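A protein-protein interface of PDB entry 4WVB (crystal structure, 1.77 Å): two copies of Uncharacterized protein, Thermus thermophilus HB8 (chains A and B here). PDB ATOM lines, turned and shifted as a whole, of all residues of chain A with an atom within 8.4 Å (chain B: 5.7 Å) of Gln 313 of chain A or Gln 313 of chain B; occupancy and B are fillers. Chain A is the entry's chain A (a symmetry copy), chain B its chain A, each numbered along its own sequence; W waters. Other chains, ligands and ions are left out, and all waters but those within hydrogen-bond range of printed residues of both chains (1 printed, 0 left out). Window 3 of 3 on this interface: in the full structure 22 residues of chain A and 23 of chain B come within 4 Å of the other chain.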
ATOM      1  N   GLU A 274      -5.888  24.862 -19.813  1.00  0.00           N
ATOM      2  CA  GLU A 274      -5.707  23.387 -19.816  1.00  0.00           C
ATOM      3  C   GLU A 274      -4.392  22.928 -19.212  1.00  0.00           C
ATOM      4  O   GLU A 274      -4.287  21.813 -18.688  1.00  0.00           O
ATOM      5  CB  GLU A 274      -5.913  22.786 -21.205  1.00  0.00           C
ATOM      6  CG  GLU A 274      -7.376  22.857 -21.608  1.00  0.00           C
ATOM      7  CD  GLU A 274      -8.223  21.982 -20.690  1.00  0.00           C
ATOM      8  OE1 GLU A 274      -8.048  20.755 -20.752  1.00  0.00           O
ATOM      9  OE2 GLU A 274      -8.973  22.550 -19.878  1.00  0.00           O
ATOM     10  N   LEU A 306     -14.861  23.931 -16.436  1.00  0.00           N
ATOM     11  CA  LEU A 306     -16.083  23.488 -17.146  1.00  0.00           C
ATOM     12  C   LEU A 306     -16.921  24.683 -17.678  1.00  0.00           C
ATOM     13  O   LEU A 306     -17.470  24.642 -18.785  1.00  0.00           O
ATOM     14  CB  LEU A 306     -16.943  22.642 -16.217  1.00  0.00           C
ATOM     15  CG  LEU A 306     -16.304  21.348 -15.717  1.00  0.00           C
ATOM     16  CD1 LEU A 306     -17.063  20.917 -14.461  1.00  0.00           C
ATOM     17  CD2 LEU A 306     -16.367  20.263 -16.758  1.00  0.00           C
ATOM     18  N   GLY A 309     -15.359  26.026 -20.689  1.00  0.00           N
ATOM     19  CA  GLY A 309     -15.538  25.178 -21.838  1.00  0.00           C
ATOM     20  C   GLY A 309     -14.257  24.620 -22.461  1.00  0.00           C
ATOM     21  O   GLY A 309     -14.274  24.209 -23.628  1.00  0.00           O
ATOM     22  N   THR A 310     -13.168  24.576 -21.696  1.00  0.00           N
ATOM     23  CA  THR A 310     -11.867  24.099 -22.183  1.00  0.00           C
ATOM     24  C   THR A 310     -11.555  22.589 -22.096  1.00  0.00           C
ATOM     25  O   THR A 310     -10.892  22.063 -22.984  1.00  0.00           O
ATOM     26  CB  THR A 310     -10.702  24.891 -21.529  1.00  0.00           C
ATOM     27  OG1 THR A 310     -10.617  24.602 -20.133  1.00  0.00           O
ATOM     28  CG2 THR A 310     -10.907  26.386 -21.730  1.00  0.00           C
ATOM     29  N   PRO A 311     -12.032  21.886 -21.060  1.00  0.00           N
ATOM     30  CA  PRO A 311     -11.685  20.456 -21.097  1.00  0.00           C
ATOM     31  C   PRO A 311     -12.331  19.658 -22.223  1.00  0.00           C
ATOM     32  O   PRO A 311     -13.355  20.065 -22.787  1.00  0.00           O
ATOM     33  CB  PRO A 311     -12.217  19.910 -19.764  1.00  0.00           C
ATOM     34  CG  PRO A 311     -13.139  20.917 -19.263  1.00  0.00           C
ATOM     35  CD  PRO A 311     -12.784  22.252 -19.845  1.00  0.00           C
ATOM     36  N   HIS A 312     -11.729  18.516 -22.530  1.00  0.00           N
ATOM     37  CA  HIS A 312     -12.429  17.521 -23.326  1.00  0.00           C
ATOM     38  C   HIS A 312     -13.337  16.714 -22.362  1.00  0.00           C
ATOM     39  O   HIS A 312     -13.263  16.848 -21.135  1.00  0.00           O
ATOM     40  CB  HIS A 312     -11.476  16.645 -24.166  1.00  0.00           C
ATOM     41  CG  HIS A 312     -10.444  15.893 -23.383  1.00  0.00           C
ATOM     42  ND1 HIS A 312     -10.771  14.947 -22.440  1.00  0.00           N
ATOM     43  CD2 HIS A 312      -9.089  15.863 -23.483  1.00  0.00           C
ATOM     44  CE1 HIS A 312      -9.670  14.400 -21.951  1.00  0.00           C
ATOM     45  NE2 HIS A 312      -8.634  14.946 -22.561  1.00  0.00           N
ATOM     46  N   GLN A 313     -14.191  15.905 -22.943  1.00  0.00           N
ATOM     47  CA  GLN A 313     -15.228  15.209 -22.171  1.00  0.00           C
ATOM     48  C   GLN A 313     -14.677  14.218 -21.149  1.00  0.00           C
ATOM     49  O   GLN A 313     -15.248  14.043 -20.073  1.00  0.00           O
ATOM     50  CB  GLN A 313     -16.130  14.448 -23.123  1.00  0.00           C
ATOM     51  CG  GLN A 313     -17.359  13.826 -22.488  1.00  0.00           C
ATOM     52  CD  GLN A 313     -18.303  14.840 -21.951  1.00  0.00           C
ATOM     53  OE1 GLN A 313     -19.165  14.523 -21.132  1.00  0.00           O
ATOM     54  NE2 GLN A 313     -18.209  16.063 -22.448  1.00  0.00           N
ATOM     55  N   GLY A 314     -13.600  13.538 -21.497  1.00  0.00           N
ATOM     56  CA  GLY A 314     -12.945  12.620 -20.561  1.00  0.00           C
ATOM     57  C   GLY A 314     -12.517  13.325 -19.300  1.00  0.00           C
ATOM     58  O   GLY A 314     -12.708  12.833 -18.180  1.00  0.00           O
ATOM     59  N   ARG A 315     -11.947  14.515 -19.473  1.00  0.00           N
ATOM     60  CA  ARG A 315     -11.541  15.333 -18.370  1.00  0.00           C
ATOM     61  C   ARG A 315     -12.750  15.837 -17.539  1.00  0.00           C
ATOM     62  O   ARG A 315     -12.733  15.788 -16.302  1.00  0.00           O
ATOM     63  CB  ARG A 315     -10.739  16.503 -18.927  1.00  0.00           C
ATOM     64  CG  ARG A 315     -10.002  17.299 -17.903  1.00  0.00           C
ATOM     65  CD  ARG A 315      -8.813  18.027 -18.560  1.00  0.00           C
ATOM     66  NE  ARG A 315      -7.748  17.102 -18.907  1.00  0.00           N
ATOM     67  CZ  ARG A 315      -6.578  17.444 -19.435  1.00  0.00           C
ATOM     68  NH1 ARG A 315      -6.279  18.725 -19.662  1.00  0.00           N
ATOM     69  NH2 ARG A 315      -5.676  16.491 -19.678  1.00  0.00           N
ATOM     70  N   ALA A 316     -13.802  16.278 -18.227  1.00  0.00           N
ATOM     71  CA  ALA A 316     -15.055  16.637 -17.579  1.00  0.00           C
ATOM     72  C   ALA A 316     -15.615  15.442 -16.773  1.00  0.00           C
ATOM     73  O   ALA A 316     -16.161  15.628 -15.688  1.00  0.00           O
ATOM     74  CB  ALA A 316     -16.064  17.089 -18.610  1.00  0.00           C
ATOM     75  N   SER A 317     -15.476  14.233 -17.320  1.00  0.00           N
ATOM     76  CA  SER A 317     -15.985  13.022 -16.645  1.00  0.00           C
ATOM     77  C   SER A 317     -15.194  12.732 -15.360  1.00  0.00           C
ATOM     78  O   SER A 317     -15.772  12.358 -14.321  1.00  0.00           O
ATOM     79  CB  SER A 317     -16.029  11.828 -17.606  1.00  0.00           C
ATOM     80  OG  SER A 317     -14.810  11.110 -17.596  1.00  0.00           O
ATOM     81  N   LEU A 318     -13.881  12.994 -15.383  1.00  0.00           N
ATOM     82  CA  LEU A 318     -13.087  12.845 -14.191  1.00  0.00           C
ATOM     83  C   LEU A 318     -13.471  13.870 -13.147  1.00  0.00           C
ATOM     84  O   LEU A 318     -13.463  13.559 -11.955  1.00  0.00           O
ATOM     85  CB  LEU A 318     -11.595  12.881 -14.509  1.00  0.00           C
ATOM     86  CG  LEU A 318     -11.091  11.727 -15.386  1.00  0.00           C
ATOM     87  CD1 LEU A 318      -9.696  12.043 -15.901  1.00  0.00           C
ATOM     88  CD2 LEU A 318     -11.106  10.379 -14.660  1.00  0.00           C
ATOM     89  N   LEU A 319     -13.815  15.091 -13.572  1.00  0.00           N
ATOM     90  CA  LEU A 319     -14.355  16.080 -12.644  1.00  0.00           C
ATOM     91  C   LEU A 319     -15.704  15.660 -12.093  1.00  0.00           C
ATOM     92  O   LEU A 319     -15.957  15.849 -10.908  1.00  0.00           O
ATOM     93  CB  LEU A 319     -14.481  17.454 -13.267  1.00  0.00           C
ATOM     94  CG  LEU A 319     -13.107  18.144 -13.437  1.00  0.00           C
ATOM     95  CD1 LEU A 319     -13.377  19.461 -14.140  1.00  0.00           C
ATOM     96  CD2 LEU A 319     -12.365  18.374 -12.126  1.00  0.00           C
ATOM     97  N   ALA A 320     -16.550  15.089 -12.937  1.00  0.00           N
ATOM     98  CA  ALA A 320     -17.883  14.682 -12.465  1.00  0.00           C
ATOM     99  C   ALA A 320     -17.713  13.607 -11.402  1.00  0.00           C
ATOM    100  O   ALA A 320     -18.396  13.639 -10.361  1.00  0.00           O
ATOM    101  CB  ALA A 320     -18.725  14.168 -13.620  1.00  0.00           C
ATOM    102  N   GLN A 321     -16.800  12.667 -11.647  1.00  0.00           N
ATOM    103  CA  GLN A 321     -16.497  11.614 -10.658  1.00  0.00           C
ATOM    104  C   GLN A 321     -16.006  12.188  -9.350  1.00  0.00           C
ATOM    105  O   GLN A 321     -16.407  11.722  -8.268  1.00  0.00           O
ATOM    106  CB  GLN A 321     -15.476  10.605 -11.199  1.00  0.00           C
ATOM    107  CG  GLN A 321     -16.019   9.763 -12.331  1.00  0.00           C
ATOM    108  CD  GLN A 321     -14.943   9.024 -13.117  1.00  0.00           C
ATOM    109  OE1 GLN A 321     -15.133   8.709 -14.288  1.00  0.00           O
ATOM    110  NE2 GLN A 321     -13.813   8.759 -12.486  1.00  0.00           N
ATOM    111  N   GLY A 365     -21.508  24.675 -16.125  1.00  0.00           N
ATOM    112  CA  GLY A 365     -20.450  23.933 -16.803  1.00  0.00           C
ATOM    113  C   GLY A 365     -20.748  22.450 -16.974  1.00  0.00           C
ATOM    114  O   GLY A 365     -20.599  21.886 -18.068  1.00  0.00           O
ATOM    115  N   PHE A 366     -21.208  21.802 -15.896  1.00  0.00           N
ATOM    116  CA  PHE A 366     -21.538  20.391 -16.005  1.00  0.00           C
ATOM    117  C   PHE A 366     -22.625  20.142 -17.039  1.00  0.00           C
ATOM    118  O   PHE A 366     -22.518  19.190 -17.819  1.00  0.00           O
ATOM    119  CB  PHE A 366     -21.920  19.795 -14.630  1.00  0.00           C
ATOM    120  CG  PHE A 366     -20.736  19.277 -13.857  1.00  0.00           C
ATOM    121  CD1 PHE A 366     -19.888  18.337 -14.424  1.00  0.00           C
ATOM    122  CD2 PHE A 366     -20.454  19.736 -12.577  1.00  0.00           C
ATOM    123  CE1 PHE A 366     -18.804  17.846 -13.731  1.00  0.00           C
ATOM    124  CE2 PHE A 366     -19.362  19.260 -11.871  1.00  0.00           C
ATOM    125  CZ  PHE A 366     -18.530  18.308 -12.439  1.00  0.00           C
ATOM    126  N   ARG A 367     -23.637  20.994 -17.053  1.00  0.00           N
ATOM    127  CA  ARG A 367     -24.745  20.891 -18.027  1.00  0.00           C
ATOM    128  C   ARG A 367     -24.217  20.944 -19.444  1.00  0.00           C
ATOM    129  O   ARG A 367     -24.602  20.148 -20.314  1.00  0.00           O
ATOM    130  CB  ARG A 367     -25.771  22.004 -17.821  1.00  0.00           C
ATOM    131  CG  ARG A 367     -27.009  21.942 -18.731  1.00  0.00           C
ATOM    132  CD  ARG A 367     -26.826  22.537 -20.149  1.00  0.00           C
ATOM    133  NE  ARG A 367     -26.044  23.781 -20.122  1.00  0.00           N
ATOM    134  CZ  ARG A 367     -26.499  24.986 -19.768  1.00  0.00           C
ATOM    135  NH1 ARG A 367     -27.789  25.165 -19.482  1.00  0.00           N
ATOM    136  NH2 ARG A 367     -25.654  26.038 -19.724  1.00  0.00           N
ATOM    137  N   ASP A 368     -23.310  21.891 -19.676  1.00  0.00           N
ATOM    138  CA  ASP A 368     -22.644  22.000 -20.986  1.00  0.00           C
ATOM    139  C   ASP A 368     -21.922  20.747 -21.458  1.00  0.00           C
ATOM    140  O   ASP A 368     -21.847  20.484 -22.657  1.00  0.00           O
ATOM    141  CB  ASP A 368     -21.672  23.186 -20.979  1.00  0.00           C
ATOM    142  CG  ASP A 368     -22.355  24.505 -20.823  1.00  0.00           C
ATOM    143  OD1 ASP A 368     -23.588  24.610 -21.023  1.00  0.00           O
ATOM    144  OD2 ASP A 368     -21.634  25.491 -20.504  1.00  0.00           O
ATOM    145  N   TYR A 369     -21.404  19.960 -20.527  1.00  0.00           N
ATOM    146  CA  TYR A 369     -20.732  18.720 -20.842  1.00  0.00           C
ATOM    147  C   TYR A 369     -21.660  17.484 -20.756  1.00  0.00           C
ATOM    148  O   TYR A 369     -21.204  16.347 -20.801  1.00  0.00           O
ATOM    149  CB  TYR A 369     -19.510  18.568 -19.936  1.00  0.00           C
ATOM    150  CG  TYR A 369     -18.363  19.443 -20.418  1.00  0.00           C
ATOM    151  CD1 TYR A 369     -18.247  20.747 -20.012  1.00  0.00           C
ATOM    152  CD2 TYR A 369     -17.441  18.952 -21.328  1.00  0.00           C
ATOM    153  CE1 TYR A 369     -17.204  21.551 -20.500  1.00  0.00           C
ATOM    154  CE2 TYR A 369     -16.395  19.716 -21.804  1.00  0.00           C
ATOM    155  CZ  TYR A 369     -16.282  21.018 -21.379  1.00  0.00           C
ATOM    156  OH  TYR A 369     -15.253  21.784 -21.889  1.00  0.00           O
ATOM    157  N   GLY A 370     -22.957  17.731 -20.666  1.00  0.00           N
ATOM    158  CA  GLY A 370     -23.932  16.641 -20.678  1.00  0.00           C
ATOM    159  C   GLY A 370     -24.206  16.016 -19.321  1.00  0.00           C
ATOM    160  O   GLY A 370     -24.957  14.995 -19.253  1.00  0.00           O
ATOM    161  N   PHE A 371     -23.640  16.568 -18.240  1.00  0.00           N
ATOM    162  CA  PHE A 371     -23.840  15.967 -16.900  1.00  0.00           C
ATOM    163  C   PHE A 371     -25.099  16.558 -16.265  1.00  0.00           C
ATOM    164  O   PHE A 371     -25.058  17.333 -15.305  1.00  0.00           O
ATOM    165  CB  PHE A 371     -22.593  16.074 -16.026  1.00  0.00           C
ATOM    166  CG  PHE A 371     -21.437  15.283 -16.557  1.00  0.00           C
ATOM    167  CD1 PHE A 371     -21.292  13.936 -16.251  1.00  0.00           C
ATOM    168  CD2 PHE A 371     -20.533  15.856 -17.422  1.00  0.00           C
ATOM    169  CE1 PHE A 371     -20.239  13.183 -16.766  1.00  0.00           C
ATOM    170  CE2 PHE A 371     -19.487  15.109 -17.944  1.00  0.00           C
ATOM    171  CZ  PHE A 371     -19.330  13.779 -17.620  1.00  0.00           C
ATOM    172  N   PRO B 311     -17.411  20.741 -32.068  1.00  0.00           N
ATOM    173  CA  PRO B 311     -17.851  20.574 -30.673  1.00  0.00           C
ATOM    174  C   PRO B 311     -17.028  19.595 -29.843  1.00  0.00           C
ATOM    175  O   PRO B 311     -16.333  18.725 -30.387  1.00  0.00           O
ATOM    176  CB  PRO B 311     -19.273  20.010 -30.798  1.00  0.00           C
ATOM    177  CG  PRO B 311     -19.393  19.537 -32.168  1.00  0.00           C
ATOM    178  CD  PRO B 311     -18.418  20.273 -33.037  1.00  0.00           C
ATOM    179  N   HIS B 312     -17.126  19.739 -28.528  1.00  0.00           N
ATOM    180  CA  HIS B 312     -16.679  18.672 -27.649  1.00  0.00           C
ATOM    181  C   HIS B 312     -17.828  17.635 -27.560  1.00  0.00           C
ATOM    182  O   HIS B 312     -18.946  17.861 -28.037  1.00  0.00           O
ATOM    183  CB  HIS B 312     -16.197  19.189 -26.276  1.00  0.00           C
ATOM    184  CG  HIS B 312     -17.210  19.967 -25.496  1.00  0.00           C
ATOM    185  ND1 HIS B 312     -18.401  19.423 -25.073  1.00  0.00           N
ATOM    186  CD2 HIS B 312     -17.163  21.215 -24.960  1.00  0.00           C
ATOM    187  CE1 HIS B 312     -19.071  20.310 -24.356  1.00  0.00           C
ATOM    188  NE2 HIS B 312     -18.346  21.411 -24.281  1.00  0.00           N
ATOM    189  N   GLN B 313     -17.518  16.507 -26.965  1.00  0.00           N
ATOM    190  CA  GLN B 313     -18.445  15.368 -26.960  1.00  0.00           C
ATOM    191  C   GLN B 313     -19.749  15.637 -26.214  1.00  0.00           C
ATOM    192  O   GLN B 313     -20.807  15.140 -26.599  1.00  0.00           O
ATOM    193  CB  GLN B 313     -17.769  14.178 -26.309  1.00  0.00           C
ATOM    194  CG  GLN B 313     -18.537  12.874 -26.393  1.00  0.00           C
ATOM    195  CD  GLN B 313     -18.688  12.386 -27.789  1.00  0.00           C
ATOM    196  OE1 GLN B 313     -19.541  11.545 -28.071  1.00  0.00           O
ATOM    197  NE2 GLN B 313     -17.823  12.848 -28.677  1.00  0.00           N
ATOM    198  N   GLY B 314     -19.673  16.380 -25.125  1.00  0.00           N
ATOM    199  CA  GLY B 314     -20.874  16.763 -24.379  1.00  0.00           C
ATOM    200  C   GLY B 314     -21.848  17.519 -25.245  1.00  0.00           C
ATOM    201  O   GLY B 314     -23.061  17.273 -25.232  1.00  0.00           O
ATOM    202  N   ARG B 315     -21.313  18.443 -26.040  1.00  0.00           N
ATOM    203  CA  ARG B 315     -22.099  19.202 -26.964  1.00  0.00           C
ATOM    204  C   ARG B 315     -22.687  18.318 -28.095  1.00  0.00           C
ATOM    205  O   ARG B 315     -23.873  18.430 -28.436  1.00  0.00           O
ATOM    206  CB  ARG B 315     -21.215  20.302 -27.537  1.00  0.00           C
ATOM    207  CG  ARG B 315     -21.944  21.357 -28.301  1.00  0.00           C
ATOM    208  CD  ARG B 315     -21.119  22.658 -28.316  1.00  0.00           C
ATOM    209  NE  ARG B 315     -21.122  23.306 -27.017  1.00  0.00           N
ATOM    210  CZ  ARG B 315     -20.544  24.471 -26.740  1.00  0.00           C
ATOM    211  NH1 ARG B 315     -19.920  25.167 -27.692  1.00  0.00           N
ATOM    212  NH2 ARG B 315     -20.650  24.966 -25.505  1.00  0.00           N
ATOM    213  N   ALA B 316     -21.864  17.424 -28.639  1.00  0.00           N
ATOM    214  CA  ALA B 316     -22.325  16.433 -29.601  1.00  0.00           C
ATOM    215  C   ALA B 316     -23.460  15.573 -28.998  1.00  0.00           C
ATOM    216  O   ALA B 316     -24.409  15.224 -29.696  1.00  0.00           O
ATOM    217  CB  ALA B 316     -21.176  15.551 -30.031  1.00  0.00           C
ATOM    218  N   SER B 317     -23.341  15.240 -27.711  1.00  0.00           N
ATOM    219  CA  SER B 317     -24.359  14.412 -27.036  1.00  0.00           C
ATOM    220  C   SER B 317     -25.690  15.168 -26.904  1.00  0.00           C
ATOM    221  O   SER B 317     -26.778  14.593 -27.106  1.00  0.00           O
ATOM    222  CB  SER B 317     -23.838  13.875 -25.696  1.00  0.00           C
ATOM    223  OG  SER B 317     -24.116  14.770 -24.637  1.00  0.00           O
ATOM    224  N   LEU B 318     -25.620  16.483 -26.666  1.00  0.00           N
ATOM    225  CA  LEU B 318     -26.817  17.283 -26.628  1.00  0.00           C
ATOM    226  C   LEU B 318     -27.459  17.368 -27.995  1.00  0.00           C
ATOM    227  O   LEU B 318     -28.687  17.377 -28.093  1.00  0.00           O
ATOM    228  CB  LEU B 318     -26.546  18.662 -26.035  1.00  0.00           C
ATOM    229  CG  LEU B 318     -26.107  18.659 -24.563  1.00  0.00           C
ATOM    230  CD1 LEU B 318     -25.556  20.026 -24.189  1.00  0.00           C
ATOM    231  CD2 LEU B 318     -27.232  18.250 -23.610  1.00  0.00           C
ATOM    232  N   TYR B 369     -18.280  11.365 -33.843  1.00  0.00           N
ATOM    233  CA  TYR B 369     -18.404  11.541 -32.413  1.00  0.00           C
ATOM    234  C   TYR B 369     -18.863  10.258 -31.679  1.00  0.00           C
ATOM    235  O   TYR B 369     -19.202  10.292 -30.501  1.00  0.00           O
ATOM    236  CB  TYR B 369     -19.344  12.714 -32.133  1.00  0.00           C
ATOM    237  CG  TYR B 369     -18.636  14.042 -32.349  1.00  0.00           C
ATOM    238  CD1 TYR B 369     -18.598  14.634 -33.585  1.00  0.00           C
ATOM    239  CD2 TYR B 369     -17.961  14.654 -31.305  1.00  0.00           C
ATOM    240  CE1 TYR B 369     -17.905  15.840 -33.773  1.00  0.00           C
ATOM    241  CE2 TYR B 369     -17.292  15.851 -31.460  1.00  0.00           C
ATOM    242  CZ  TYR B 369     -17.272  16.440 -32.701  1.00  0.00           C
ATOM    243  OH  TYR B 369     -16.570  17.619 -32.854  1.00  0.00           O
ATOM    244  N   GLY B 370     -18.830   9.137 -32.382  1.00  0.00           N
ATOM    245  CA  GLY B 370     -19.148   7.852 -31.761  1.00  0.00           C
ATOM    246  C   GLY B 370     -20.626   7.504 -31.733  1.00  0.00           C
ATOM    247  O   GLY B 370     -21.003   6.459 -31.119  1.00  0.00           O
ATOM    248  N   PHE B 371     -21.483   8.319 -32.360  1.00  0.00           N
ATOM    249  CA  PHE B 371     -22.940   8.048 -32.321  1.00  0.00           C
ATOM    250  C   PHE B 371     -23.313   7.130 -33.486  1.00  0.00           C
ATOM    251  O   PHE B 371     -23.969   7.521 -34.456  1.00  0.00           O
ATOM    252  CB  PHE B 371     -23.766   9.330 -32.251  1.00  0.00           C
ATOM    253  CG  PHE B 371     -23.554  10.093 -30.978  1.00  0.00           C
ATOM    254  CD1 PHE B 371     -24.287   9.795 -29.837  1.00  0.00           C
ATOM    255  CD2 PHE B 371     -22.575  11.056 -30.894  1.00  0.00           C
ATOM    256  CE1 PHE B 371     -24.073  10.476 -28.639  1.00  0.00           C
ATOM    257  CE2 PHE B 371     -22.354  11.732 -29.702  1.00  0.00           C
ATOM    258  CZ  PHE B 371     -23.099  11.453 -28.576  1.00  0.00           C
HETATM  259  O   HOH W   1     -22.391  22.413 -24.519  1.00  0.00           O
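The backbone NH of Gly 314 of chain B lies close to the side-chain amide nitrogen of Gln 313 of chain A, 3.1 Å away.
A ring nitrogen (ND1) of His 312 of chain B is in hydrogen-bond range of the backbone NH of Arg 315 of chain B. The side-chain carboxylate (OD1) of Asp 368 of chain A lies within salt-bridge range of the guanidinium group (NE) of Arg 367 of chain A, 2.7 Å away. O of Gly 309 of chain A sits close to OH of Tyr 369 of chain A (3.1 Å). OE1 of Gln 313 of chain B sits close to O of Tyr 369 of chain B (2.8 Å). The backbone carbonyl oxygen of Pro 311 of chain A is in hydrogen-bond range of the side-chain hydroxyl of Tyr 369 of chain A (2.7 Å). O of Gly 314 of chain B sits at hydrogen-bond distance from OG of Ser 317 of chain B (2.8 Å).
Among the printed residues, merely in contact across the chains: Asp 368 of chain A with His 312 of chain B (3.3 Å), Tyr 369 of chain A with His 312 of chain B (3.6 Å), Gln 313 of chain A with Gln 313 of chain B (3.6 Å), Tyr 369 of chain A with Gly 314 of chain B (3.6 Å), Asp 368 of chain A with Gly 314 of chain B (3.9 Å), Asp 368 of chain A with Arg 315 of chain B (3.99 Å) and Arg 367 of chain A with Leu 318 of chain B (3.99 Å).
Gln 313 of chain A touches two residues of chain B. Arg 315 of chain A touches none of the printed residues of chain B. Printed residues of chain B within 4 Å of Arg 367 of chain A: Leu 318. Of the printed residues of chain B, Asp 368 of chain A touches His 312, Gly 314 and Arg 315. Printed residues of chain A within 4 Å of His 312 of chain B: Asp 368 and Tyr 369. Gln 313 of chain B touches just one residue of chain A: Gln 313. Gly 314 of chain B touches just these residues of chain A: Gln 313 (3.1 Å), Asp 368 (3.9 Å) and Tyr 369 (3.6 Å). The nearest residue of chain B that does not touch Gln 313 of chain A is His 312 of chain B (4.3 Å). The nearest residue of chain A that does not touch Gln 313 of chain B is Tyr 369 of chain A (5.6 Å).
Printed residues of chain B that touch a printed residue of chain A: His 312, Gln 313, Gly 314, Arg 315 and Leu 318. Hydrophobic or aromatic side chains of chain B that line the printed part of chain A: His 312 and Leu 318. Of the 22 printed residues of chain A, 4 touch a printed residue of chain B. Hydrophobic or aromatic side chains of chain A that line the printed part of chain B: Tyr 369. Among the printed residues, 8 pairs touch across the chains. Among the printed residues, no Asp or Glu carboxylate lies within 4 Å of a Lys or Arg side-chain nitrogen of the other chain.
Gln 313 of chain A touches its own counterpart, Gln 313 of chain B. Gln 313 of chain A touches Gly 314 of chain B, but with the chains exchanged Gly 314 of chain A does not touch Gln 313 of chain B (6.4 Å). Tyr 369 of chain A touches His 312 of chain B, but with the chains exchanged His 312 of chain A does not touch Tyr 369 of chain B (9.4 Å). Tyr 369 of chain A touches Gly 314 of chain B, but with the chains exchanged Gly 314 of chain A does not touch Tyr 369 of chain B (10.8 Å). 11 positions are printed for both chains. Of the 8 pairs that touch across the chains among the printed residues, 1 has its exchanged pair printed and touching as well.
Water W1 bridges O of Asp 368 of chain A and NE of Arg 315 of chain B.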
